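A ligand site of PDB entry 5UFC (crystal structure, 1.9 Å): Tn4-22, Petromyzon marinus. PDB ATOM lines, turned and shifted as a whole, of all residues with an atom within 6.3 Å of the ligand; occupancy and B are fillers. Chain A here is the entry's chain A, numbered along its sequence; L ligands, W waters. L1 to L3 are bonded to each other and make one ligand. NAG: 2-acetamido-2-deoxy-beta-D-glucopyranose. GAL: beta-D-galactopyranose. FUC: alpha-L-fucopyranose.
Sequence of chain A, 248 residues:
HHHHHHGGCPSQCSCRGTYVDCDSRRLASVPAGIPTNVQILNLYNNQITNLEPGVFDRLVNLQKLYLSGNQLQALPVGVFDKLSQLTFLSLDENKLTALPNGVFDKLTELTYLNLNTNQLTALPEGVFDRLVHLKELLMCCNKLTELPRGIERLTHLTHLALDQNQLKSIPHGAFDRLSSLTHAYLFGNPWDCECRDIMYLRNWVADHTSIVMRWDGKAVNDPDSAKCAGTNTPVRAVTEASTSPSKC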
ATOM      1  N   TYR A  44       6.776  11.283 -30.785  1.00  0.00           N
ATOM      2  CA  TYR A  44       7.758  10.649 -29.923  1.00  0.00           C
ATOM      3  C   TYR A  44       8.986  10.084 -30.667  1.00  0.00           C
ATOM      4  O   TYR A  44       8.846   9.507 -31.734  1.00  0.00           O
ATOM      5  CB  TYR A  44       7.073   9.522 -29.127  1.00  0.00           C
ATOM      6  CG  TYR A  44       7.971   8.435 -28.591  1.00  0.00           C
ATOM      7  CD1 TYR A  44       8.865   8.677 -27.556  1.00  0.00           C
ATOM      8  CD2 TYR A  44       7.878   7.134 -29.084  1.00  0.00           C
ATOM      9  CE1 TYR A  44       9.660   7.686 -27.049  1.00  0.00           C
ATOM     10  CE2 TYR A  44       8.688   6.125 -28.585  1.00  0.00           C
ATOM     11  CZ  TYR A  44       9.571   6.410 -27.563  1.00  0.00           C
ATOM     12  OH  TYR A  44      10.373   5.402 -27.070  1.00  0.00           O
ATOM     13  N   SER A  68       7.678  13.686 -26.452  1.00  0.00           N
ATOM     14  CA  SER A  68       8.698  12.892 -25.783  1.00  0.00           C
ATOM     15  C   SER A  68       9.841  12.502 -26.718  1.00  0.00           C
ATOM     16  O   SER A  68       9.605  12.195 -27.875  1.00  0.00           O
ATOM     17  CB  SER A  68       8.092  11.614 -25.223  1.00  0.00           C
ATOM     18  OG  SER A  68       6.897  11.890 -24.519  1.00  0.00           O
ATOM     19  N   PHE A  88      -3.495  15.672 -22.423  1.00  0.00           N
ATOM     20  CA  PHE A  88      -2.261  14.914 -22.228  1.00  0.00           C
ATOM     21  C   PHE A  88      -1.102  15.619 -22.950  1.00  0.00           C
ATOM     22  O   PHE A  88      -1.168  15.818 -24.165  1.00  0.00           O
ATOM     23  CB  PHE A  88      -2.442  13.478 -22.753  1.00  0.00           C
ATOM     24  CG  PHE A  88      -1.257  12.549 -22.524  1.00  0.00           C
ATOM     25  CD1 PHE A  88      -1.356  11.476 -21.647  1.00  0.00           C
ATOM     26  CD2 PHE A  88      -0.053  12.726 -23.211  1.00  0.00           C
ATOM     27  CE1 PHE A  88      -0.277  10.611 -21.449  1.00  0.00           C
ATOM     28  CE2 PHE A  88       1.026  11.884 -23.009  1.00  0.00           C
ATOM     29  CZ  PHE A  88       0.906  10.816 -22.135  1.00  0.00           C
ATOM     30  N   SER A  90       3.186  15.322 -23.171  1.00  0.00           N
ATOM     31  CA  SER A  90       4.486  14.819 -22.724  1.00  0.00           C
ATOM     32  C   SER A  90       5.655  15.555 -23.403  1.00  0.00           C
ATOM     33  O   SER A  90       5.693  15.681 -24.623  1.00  0.00           O
ATOM     34  CB  SER A  90       4.592  13.307 -22.966  1.00  0.00           C
ATOM     35  OG  SER A  90       4.436  12.982 -24.342  1.00  0.00           O
ATOM     36  N   ASP A  92       8.868  14.872 -22.006  1.00  0.00           N
ATOM     37  CA  ASP A  92       9.963  14.195 -21.343  1.00  0.00           C
ATOM     38  C   ASP A  92      11.062  13.823 -22.338  1.00  0.00           C
ATOM     39  O   ASP A  92      10.801  13.709 -23.520  1.00  0.00           O
ATOM     40  CB  ASP A  92       9.465  12.950 -20.595  1.00  0.00           C
ATOM     41  CG  ASP A  92       8.596  12.040 -21.456  1.00  0.00           C
ATOM     42  OD1 ASP A  92       7.598  12.530 -22.039  1.00  0.00           O
ATOM     43  OD2 ASP A  92       8.907  10.819 -21.528  1.00  0.00           O
ATOM     44  N   GLU A  93      12.266  13.632 -21.825  1.00  0.00           N
ATOM     45  CA  GLU A  93      13.471  13.379 -22.633  1.00  0.00           C
ATOM     46  C   GLU A  93      13.642  14.384 -23.761  1.00  0.00           C
ATOM     47  O   GLU A  93      13.688  14.026 -24.937  1.00  0.00           O
ATOM     48  CB  GLU A  93      13.459  11.944 -23.180  1.00  0.00           C
ATOM     49  CG  GLU A  93      13.573  10.897 -22.073  1.00  0.00           C
ATOM     50  CD  GLU A  93      13.682   9.460 -22.622  1.00  0.00           C
ATOM     51  OE1 GLU A  93      14.512   9.222 -23.514  1.00  0.00           O
ATOM     52  OE2 GLU A  93      12.924   8.584 -22.156  1.00  0.00           O
ATOM     53  N   TYR A 112      -2.617  15.320 -17.523  1.00  0.00           N
ATOM     54  CA  TYR A 112      -1.318  14.634 -17.546  1.00  0.00           C
ATOM     55  C   TYR A 112      -0.247  15.549 -18.101  1.00  0.00           C
ATOM     56  O   TYR A 112      -0.370  16.025 -19.224  1.00  0.00           O
ATOM     57  CB  TYR A 112      -1.406  13.351 -18.394  1.00  0.00           C
ATOM     58  CG  TYR A 112      -0.088  12.563 -18.460  1.00  0.00           C
ATOM     59  CD1 TYR A 112       0.133  11.483 -17.599  1.00  0.00           C
ATOM     60  CD2 TYR A 112       0.907  12.885 -19.375  1.00  0.00           C
ATOM     61  CE1 TYR A 112       1.326  10.766 -17.647  1.00  0.00           C
ATOM     62  CE2 TYR A 112       2.094  12.178 -19.430  1.00  0.00           C
ATOM     63  CZ  TYR A 112       2.297  11.112 -18.574  1.00  0.00           C
ATOM     64  OH  TYR A 112       3.478  10.415 -18.638  1.00  0.00           O
ATOM     65  N   ASN A 114       4.060  15.676 -18.399  1.00  0.00           N
ATOM     66  CA  ASN A 114       5.345  15.008 -18.175  1.00  0.00           C
ATOM     67  C   ASN A 114       6.527  15.849 -18.656  1.00  0.00           C
ATOM     68  O   ASN A 114       6.695  16.061 -19.860  1.00  0.00           O
ATOM     69  CB  ASN A 114       5.360  13.645 -18.901  1.00  0.00           C
ATOM     70  CG  ASN A 114       6.496  12.722 -18.430  1.00  0.00           C
ATOM     71  OD1 ASN A 114       7.517  13.180 -17.926  1.00  0.00           O
ATOM     72  ND2 ASN A 114       6.298  11.404 -18.580  1.00  0.00           N
ATOM     73  N   ASN A 116       9.694  14.999 -17.287  1.00  0.00           N
ATOM     74  CA  ASN A 116      10.850  14.157 -16.890  1.00  0.00           C
ATOM     75  C   ASN A 116      12.046  14.322 -17.825  1.00  0.00           C
ATOM     76  O   ASN A 116      11.861  14.442 -19.015  1.00  0.00           O
ATOM     77  CB  ASN A 116      10.487  12.660 -16.885  1.00  0.00           C
ATOM     78  CG  ASN A 116       9.659  12.234 -15.673  1.00  0.00           C
ATOM     79  OD1 ASN A 116       9.343  13.025 -14.790  1.00  0.00           O
ATOM     80  ND2 ASN A 116       9.323  10.940 -15.642  1.00  0.00           N
ATOM     81  N   THR A 117      13.256  14.238 -17.268  1.00  0.00           N
ATOM     82  CA  THR A 117      14.482  14.170 -18.045  1.00  0.00           C
ATOM     83  C   THR A 117      14.624  15.357 -19.009  1.00  0.00           C
ATOM     84  O   THR A 117      14.653  15.227 -20.234  1.00  0.00           O
ATOM     85  CB  THR A 117      14.550  12.818 -18.794  1.00  0.00           C
ATOM     86  OG1 THR A 117      14.371  11.771 -17.827  1.00  0.00           O
ATOM     87  CG2 THR A 117      15.904  12.607 -19.493  1.00  0.00           C
ATOM     88  N   LEU A 138       4.795  14.912 -13.616  1.00  0.00           N
ATOM     89  CA  LEU A 138       6.081  14.223 -13.545  1.00  0.00           C
ATOM     90  C   LEU A 138       7.176  15.201 -13.927  1.00  0.00           C
ATOM     91  O   LEU A 138       7.122  15.826 -14.985  1.00  0.00           O
ATOM     92  CB  LEU A 138       6.085  12.990 -14.473  1.00  0.00           C
ATOM     93  CG  LEU A 138       4.870  12.052 -14.419  1.00  0.00           C
ATOM     94  CD1 LEU A 138       5.050  10.831 -15.320  1.00  0.00           C
ATOM     95  CD2 LEU A 138       4.556  11.615 -12.966  1.00  0.00           C
ATOM     96  N   MET A 139       8.175  15.378 -13.062  1.00  0.00           N
ATOM     97  CA  MET A 139       9.274  16.264 -13.426  1.00  0.00           C
ATOM     98  C   MET A 139      10.597  15.735 -12.853  1.00  0.00           C
ATOM     99  O   MET A 139      11.453  16.482 -12.402  1.00  0.00           O
ATOM    100  CB  MET A 139       8.985  17.714 -12.967  1.00  0.00           C
ATOM    101  CG  MET A 139       8.992  17.988 -11.497  1.00  0.00           C
ATOM    102  SD  MET A 139       8.229  19.597 -11.095  1.00  0.00           S
ATOM    103  CE  MET A 139       6.536  19.091 -10.884  1.00  0.00           C
ATOM    104  N   CYS A 140      10.768  14.412 -12.927  1.00  0.00           N
ATOM    105  CA  CYS A 140      12.015  13.787 -12.508  1.00  0.00           C
ATOM    106  C   CYS A 140      13.185  14.238 -13.361  1.00  0.00           C
ATOM    107  O   CYS A 140      12.994  14.749 -14.465  1.00  0.00           O
ATOM    108  CB  CYS A 140      11.926  12.262 -12.600  1.00  0.00           C
ATOM    109  SG  CYS A 140      12.780  11.567 -14.076  1.00  0.00           S
ATOM    110  N   CYS A 141      14.392  14.007 -12.840  1.00  0.00           N
ATOM    111  CA  CYS A 141      15.607  14.076 -13.635  1.00  0.00           C
ATOM    112  C   CYS A 141      15.799  15.433 -14.281  1.00  0.00           C
ATOM    113  O   CYS A 141      16.166  15.545 -15.458  1.00  0.00           O
ATOM    114  CB  CYS A 141      15.588  12.964 -14.693  1.00  0.00           C
ATOM    115  SG  CYS A 141      14.876  11.421 -14.029  1.00  0.00           S
ATOM    116  N   HIS A 159      -0.359  11.121  -9.075  1.00  0.00           N
ATOM    117  CA  HIS A 159       1.051  10.815  -9.323  1.00  0.00           C
ATOM    118  C   HIS A 159       1.864  12.084  -9.317  1.00  0.00           C
ATOM    119  O   HIS A 159       1.553  13.021 -10.044  1.00  0.00           O
ATOM    120  CB  HIS A 159       1.248  10.099 -10.674  1.00  0.00           C
ATOM    121  CG  HIS A 159       0.612   8.747 -10.762  1.00  0.00           C
ATOM    122  ND1 HIS A 159      -0.748   8.558 -10.665  1.00  0.00           N
ATOM    123  CD2 HIS A 159       1.150   7.519 -10.981  1.00  0.00           C
ATOM    124  CE1 HIS A 159      -1.023   7.276 -10.802  1.00  0.00           C
ATOM    125  NE2 HIS A 159       0.107   6.626 -10.981  1.00  0.00           N
ATOM    126  N   ALA A 161       6.048  13.016  -9.544  1.00  0.00           N
ATOM    127  CA  ALA A 161       7.421  12.556  -9.647  1.00  0.00           C
ATOM    128  C   ALA A 161       8.394  13.701  -9.501  1.00  0.00           C
ATOM    129  O   ALA A 161       8.417  14.612 -10.340  1.00  0.00           O
ATOM    130  CB  ALA A 161       7.653  11.852 -10.995  1.00  0.00           C
ATOM    131  N   LEU A 162       9.218  13.632  -8.459  1.00  0.00           N
ATOM    132  CA  LEU A 162      10.228  14.653  -8.186  1.00  0.00           C
ATOM    133  C   LEU A 162      11.623  14.034  -8.105  1.00  0.00           C
ATOM    134  O   LEU A 162      12.567  14.703  -7.692  1.00  0.00           O
ATOM    135  CB  LEU A 162       9.919  15.399  -6.878  1.00  0.00           C
ATOM    136  CG  LEU A 162       8.584  16.115  -6.778  1.00  0.00           C
ATOM    137  CD1 LEU A 162       8.327  16.572  -5.336  1.00  0.00           C
ATOM    138  CD2 LEU A 162       8.511  17.281  -7.763  1.00  0.00           C
ATOM    139  N   ASP A 163      11.743  12.759  -8.481  1.00  0.00           N
ATOM    140  CA  ASP A 163      12.987  12.038  -8.221  1.00  0.00           C
ATOM    141  C   ASP A 163      14.137  12.612  -9.041  1.00  0.00           C
ATOM    142  O   ASP A 163      13.905  13.230 -10.067  1.00  0.00           O
ATOM    143  CB  ASP A 163      12.816  10.529  -8.496  1.00  0.00           C
ATOM    144  CG  ASP A 163      12.214  10.244  -9.859  1.00  0.00           C
ATOM    145  OD1 ASP A 163      10.972  10.390 -10.026  1.00  0.00           O
ATOM    146  OD2 ASP A 163      12.981   9.869 -10.766  1.00  0.00           O
ATOM    147  N   GLN A 164      15.356  12.426  -8.533  1.00  0.00           N
ATOM    148  CA  GLN A 164      16.578  12.764  -9.280  1.00  0.00           C
ATOM    149  C   GLN A 164      16.631  14.240  -9.675  1.00  0.00           C
ATOM    150  O   GLN A 164      16.978  14.607 -10.802  1.00  0.00           O
ATOM    151  CB  GLN A 164      16.707  11.856 -10.500  1.00  0.00           C
ATOM    152  CG  GLN A 164      16.803  10.364 -10.095  1.00  0.00           C
ATOM    153  CD  GLN A 164      16.744   9.441 -11.285  1.00  0.00           C
ATOM    154  OE1 GLN A 164      17.762   9.152 -11.903  1.00  0.00           O
ATOM    155  NE2 GLN A 164      15.539   8.979 -11.636  1.00  0.00           N
ATOM    156  N   TYR A 185       7.255  10.052  -6.003  1.00  0.00           N
ATOM    157  CA  TYR A 185       8.642   9.669  -6.244  1.00  0.00           C
ATOM    158  C   TYR A 185       9.561  10.742  -5.712  1.00  0.00           C
ATOM    159  O   TYR A 185       9.526  11.887  -6.189  1.00  0.00           O
ATOM    160  CB  TYR A 185       8.896   9.444  -7.740  1.00  0.00           C
ATOM    161  CG  TYR A 185       8.006   8.407  -8.384  1.00  0.00           C
ATOM    162  CD1 TYR A 185       6.767   8.753  -8.912  1.00  0.00           C
ATOM    163  CD2 TYR A 185       8.408   7.066  -8.485  1.00  0.00           C
ATOM    164  CE1 TYR A 185       5.943   7.805  -9.516  1.00  0.00           C
ATOM    165  CE2 TYR A 185       7.581   6.109  -9.087  1.00  0.00           C
ATOM    166  CZ  TYR A 185       6.358   6.488  -9.596  1.00  0.00           C
ATOM    167  OH  TYR A 185       5.538   5.542 -10.187  1.00  0.00           O
ATOM    168  N   PHE A 187      13.054   9.744  -4.517  1.00  0.00           N
ATOM    169  CA  PHE A 187      14.431   9.250  -4.428  1.00  0.00           C
ATOM    170  C   PHE A 187      15.379  10.078  -5.306  1.00  0.00           C
ATOM    171  O   PHE A 187      14.929  10.826  -6.160  1.00  0.00           O
ATOM    172  CB  PHE A 187      14.505   7.765  -4.838  1.00  0.00           C
ATOM    173  CG  PHE A 187      14.216   7.519  -6.292  1.00  0.00           C
ATOM    174  CD1 PHE A 187      12.905   7.369  -6.745  1.00  0.00           C
ATOM    175  CD2 PHE A 187      15.260   7.440  -7.212  1.00  0.00           C
ATOM    176  CE1 PHE A 187      12.644   7.146  -8.091  1.00  0.00           C
ATOM    177  CE2 PHE A 187      14.999   7.216  -8.559  1.00  0.00           C
ATOM    178  CZ  PHE A 187      13.678   7.074  -8.996  1.00  0.00           C
ATOM    179  N   TRP A 215      11.888   3.381  -8.373  1.00  0.00           N
ATOM    180  CA  TRP A 215      11.707   2.985  -9.757  1.00  0.00           C
ATOM    181  C   TRP A 215      12.707   1.899 -10.171  1.00  0.00           C
ATOM    182  O   TRP A 215      13.861   2.197 -10.467  1.00  0.00           O
ATOM    183  CB  TRP A 215      11.835   4.205 -10.694  1.00  0.00           C
ATOM    184  CG  TRP A 215      11.433   3.894 -12.112  1.00  0.00           C
ATOM    185  CD1 TRP A 215      12.256   3.591 -13.168  1.00  0.00           C
ATOM    186  CD2 TRP A 215      10.092   3.801 -12.621  1.00  0.00           C
ATOM    187  NE1 TRP A 215      11.505   3.337 -14.297  1.00  0.00           N
ATOM    188  CE2 TRP A 215      10.175   3.457 -13.981  1.00  0.00           C
ATOM    189  CE3 TRP A 215       8.838   3.995 -12.041  1.00  0.00           C
ATOM    190  CZ2 TRP A 215       9.041   3.314 -14.780  1.00  0.00           C
ATOM    191  CZ3 TRP A 215       7.712   3.850 -12.834  1.00  0.00           C
ATOM    192  CH2 TRP A 215       7.828   3.510 -14.189  1.00  0.00           C
ATOM    193  N   GLY A 217      12.568   0.065 -12.995  1.00  0.00           N
ATOM    194  CA  GLY A 217      11.967  -0.160 -14.297  1.00  0.00           C
ATOM    195  C   GLY A 217      10.458  -0.017 -14.236  1.00  0.00           C
ATOM    196  O   GLY A 217       9.777   0.016 -15.264  1.00  0.00           O
HETATM  197  C1  NAG L   1       8.750   6.744 -20.347  1.00  0.00           C
HETATM  198  C2  NAG L   1       7.881   7.647 -19.497  1.00  0.00           C
HETATM  199  C3  NAG L   1       8.650   8.252 -18.362  1.00  0.00           C
HETATM  200  C4  NAG L   1       9.332   7.217 -17.541  1.00  0.00           C
HETATM  201  C5  NAG L   1      10.125   6.261 -18.426  1.00  0.00           C
HETATM  202  C6  NAG L   1      10.648   5.095 -17.656  1.00  0.00           C
HETATM  203  C7  NAG L   1       5.911   8.675 -20.732  1.00  0.00           C
HETATM  204  C8  NAG L   1       5.360   9.798 -21.650  1.00  0.00           C
HETATM  205  N2  NAG L   1       7.315   8.700 -20.368  1.00  0.00           N
HETATM  206  O1  NAG L   1       8.001   6.110 -21.333  1.00  0.00           O
HETATM  207  O3  NAG L   1       7.745   9.046 -17.511  1.00  0.00           O
HETATM  208  O4  NAG L   1      10.284   7.884 -16.659  1.00  0.00           O
HETATM  209  O5  NAG L   1       9.283   5.687 -19.482  1.00  0.00           O
HETATM  210  O6  NAG L   1      11.495   4.379 -18.552  1.00  0.00           O
HETATM  211  O7  NAG L   1       5.176   7.795 -20.301  1.00  0.00           O
HETATM  212  C1  GAL L   2      10.161   7.406 -15.323  1.00  0.00           C
HETATM  213  C2  GAL L   2      11.384   7.802 -14.532  1.00  0.00           C
HETATM  214  C3  GAL L   2      11.197   7.443 -13.099  1.00  0.00           C
HETATM  215  C4  GAL L   2       9.948   8.014 -12.508  1.00  0.00           C
HETATM  216  C5  GAL L   2       8.749   7.622 -13.336  1.00  0.00           C
HETATM  217  C6  GAL L   2       7.529   8.325 -12.861  1.00  0.00           C
HETATM  218  O2  GAL L   2      12.521   7.056 -15.051  1.00  0.00           O
HETATM  219  O3  GAL L   2      12.363   7.765 -12.323  1.00  0.00           O
HETATM  220  O4  GAL L   2      10.046   9.465 -12.478  1.00  0.00           O
HETATM  221  O5  GAL L   2       8.957   8.005 -14.742  1.00  0.00           O
HETATM  222  O6  GAL L   2       6.396   7.853 -13.526  1.00  0.00           O
HETATM  223  C1  FUC L   3      13.616   7.909 -15.302  1.00  0.00           C
HETATM  224  C2  FUC L   3      14.871   7.210 -14.871  1.00  0.00           C
HETATM  225  C3  FUC L   3      15.053   5.941 -15.674  1.00  0.00           C
HETATM  226  C4  FUC L   3      15.113   6.222 -17.125  1.00  0.00           C
HETATM  227  C5  FUC L   3      13.851   6.938 -17.543  1.00  0.00           C
HETATM  228  C6  FUC L   3      13.971   7.369 -18.973  1.00  0.00           C
HETATM  229  O2  FUC L   3      14.744   6.890 -13.469  1.00  0.00           O
HETATM  230  O3  FUC L   3      16.228   5.252 -15.246  1.00  0.00           O
HETATM  231  O4  FUC L   3      16.223   7.087 -17.435  1.00  0.00           O
HETATM  232  O5  FUC L   3      13.660   8.157 -16.735  1.00  0.00           O
HETATM  233  O   HOH W   1      12.828   2.723 -16.724  1.00  0.00           O
HETATM  234  O   HOH W   2      16.050   4.848 -11.825  1.00  0.00           O
HETATM  235  O   HOH W   3       5.990   7.394 -16.343  1.00  0.00           O
HETATM  236  O   HOH W   4       4.798   5.151 -19.524  1.00  0.00           O
HETATM  237  O   HOH W   5       2.547   7.424 -21.005  1.00  0.00           O
HETATM  238  O   HOH W   6      12.230  10.161 -17.862  1.00  0.00           O
HETATM  239  O   HOH W   7       4.145   6.560 -12.368  1.00  0.00           O
HETATM  240  O   HOH W   8      16.414   9.944 -17.469  1.00  0.00           O
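Merely in contact with the ligand: Cys 140, Tyr 112, Glu 93, Phe 187, Ala 161, Trp 215, Leu 138, Tyr 185, Ser 90, Thr 117, Ser 68 and Cys 141.
Hydrophobic or aromatic side chains that line the ligand: Leu 138, Ala 161, Tyr 185, Phe 187 and Trp 215.
Within 4 Å of the ligand: Ser 68, Ser 90, Asp 92, Glu 93, Tyr 112, Asn 114, Asn 116, Thr 117, Leu 138, Cys 140, Cys 141, Ala 161, Asp 163, Gln 164, Tyr 185, Phe 187 and Trp 215.
Water W6 lies within hydrogen-bond range of the side-chain hydroxyl (OG1) of Thr 117 (2.7 Å) and an oxygen (O5) of FUC L3 (2.7 Å).
Water W1 lies within hydrogen-bond range of O6 of NAG L1 (2.8 Å) and NE1 of Trp 215 (2.8 Å).
Water W7 bridges the side-chain hydroxyl of Tyr 185 (2.8 Å) and an oxygen (O6) of GAL L2 (2.8 Å).
Water W8 bridges the side-chain hydroxyl of Thr 117 and an oxygen (O4) of FUC L3.
OG of Ser 68 is in hydrogen-bond range of OG of Ser 90, at 2.7 Å.
The backbone carbonyl oxygen of Tyr 185 is in hydrogen-bond range of the backbone NH of Leu 162, 2.9 Å away.
The backbone NH (N) of Met 139 sits at hydrogen-bond distance from the side-chain amide oxygen (OD1) of Asn 116 (3.1 Å).
N of Glu 93 lies close to O of Thr 117 (3.3 Å).
The backbone carbonyl oxygen of Asn 116 sits at hydrogen-bond distance from the backbone NH of Glu 93.
The side-chain sulfur (SG) of Cys 140 forms a disulfide with the side-chain sulfur (SG) of Cys 141.
N of Asp 163 is in hydrogen-bond range of O of Tyr 185.
The side-chain amide oxygen of Asn 116 sits at hydrogen-bond distance from the backbone NH of Cys 140.
An oxygen (O5) of GAL L2 lies within hydrogen-bond range of the side-chain amide nitrogen of Asn 116 (3.1 Å).
O3 of NAG L1 sits at hydrogen-bond distance from ND2 of Asn 114, 3.0 Å away.
An oxygen (O2) of FUC L3 is in hydrogen-bond range of the side-chain amide nitrogen of Gln 164, at 2.9 Å.
An oxygen (O3) of GAL L2 is in hydrogen-bond range of the side-chain carboxylate of Asp 163, 2.7 Å away.
The side-chain carboxylate (OD2) of Asp 92 lies within hydrogen-bond range of a nitrogen (N2) of NAG L1 (2.9 Å).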
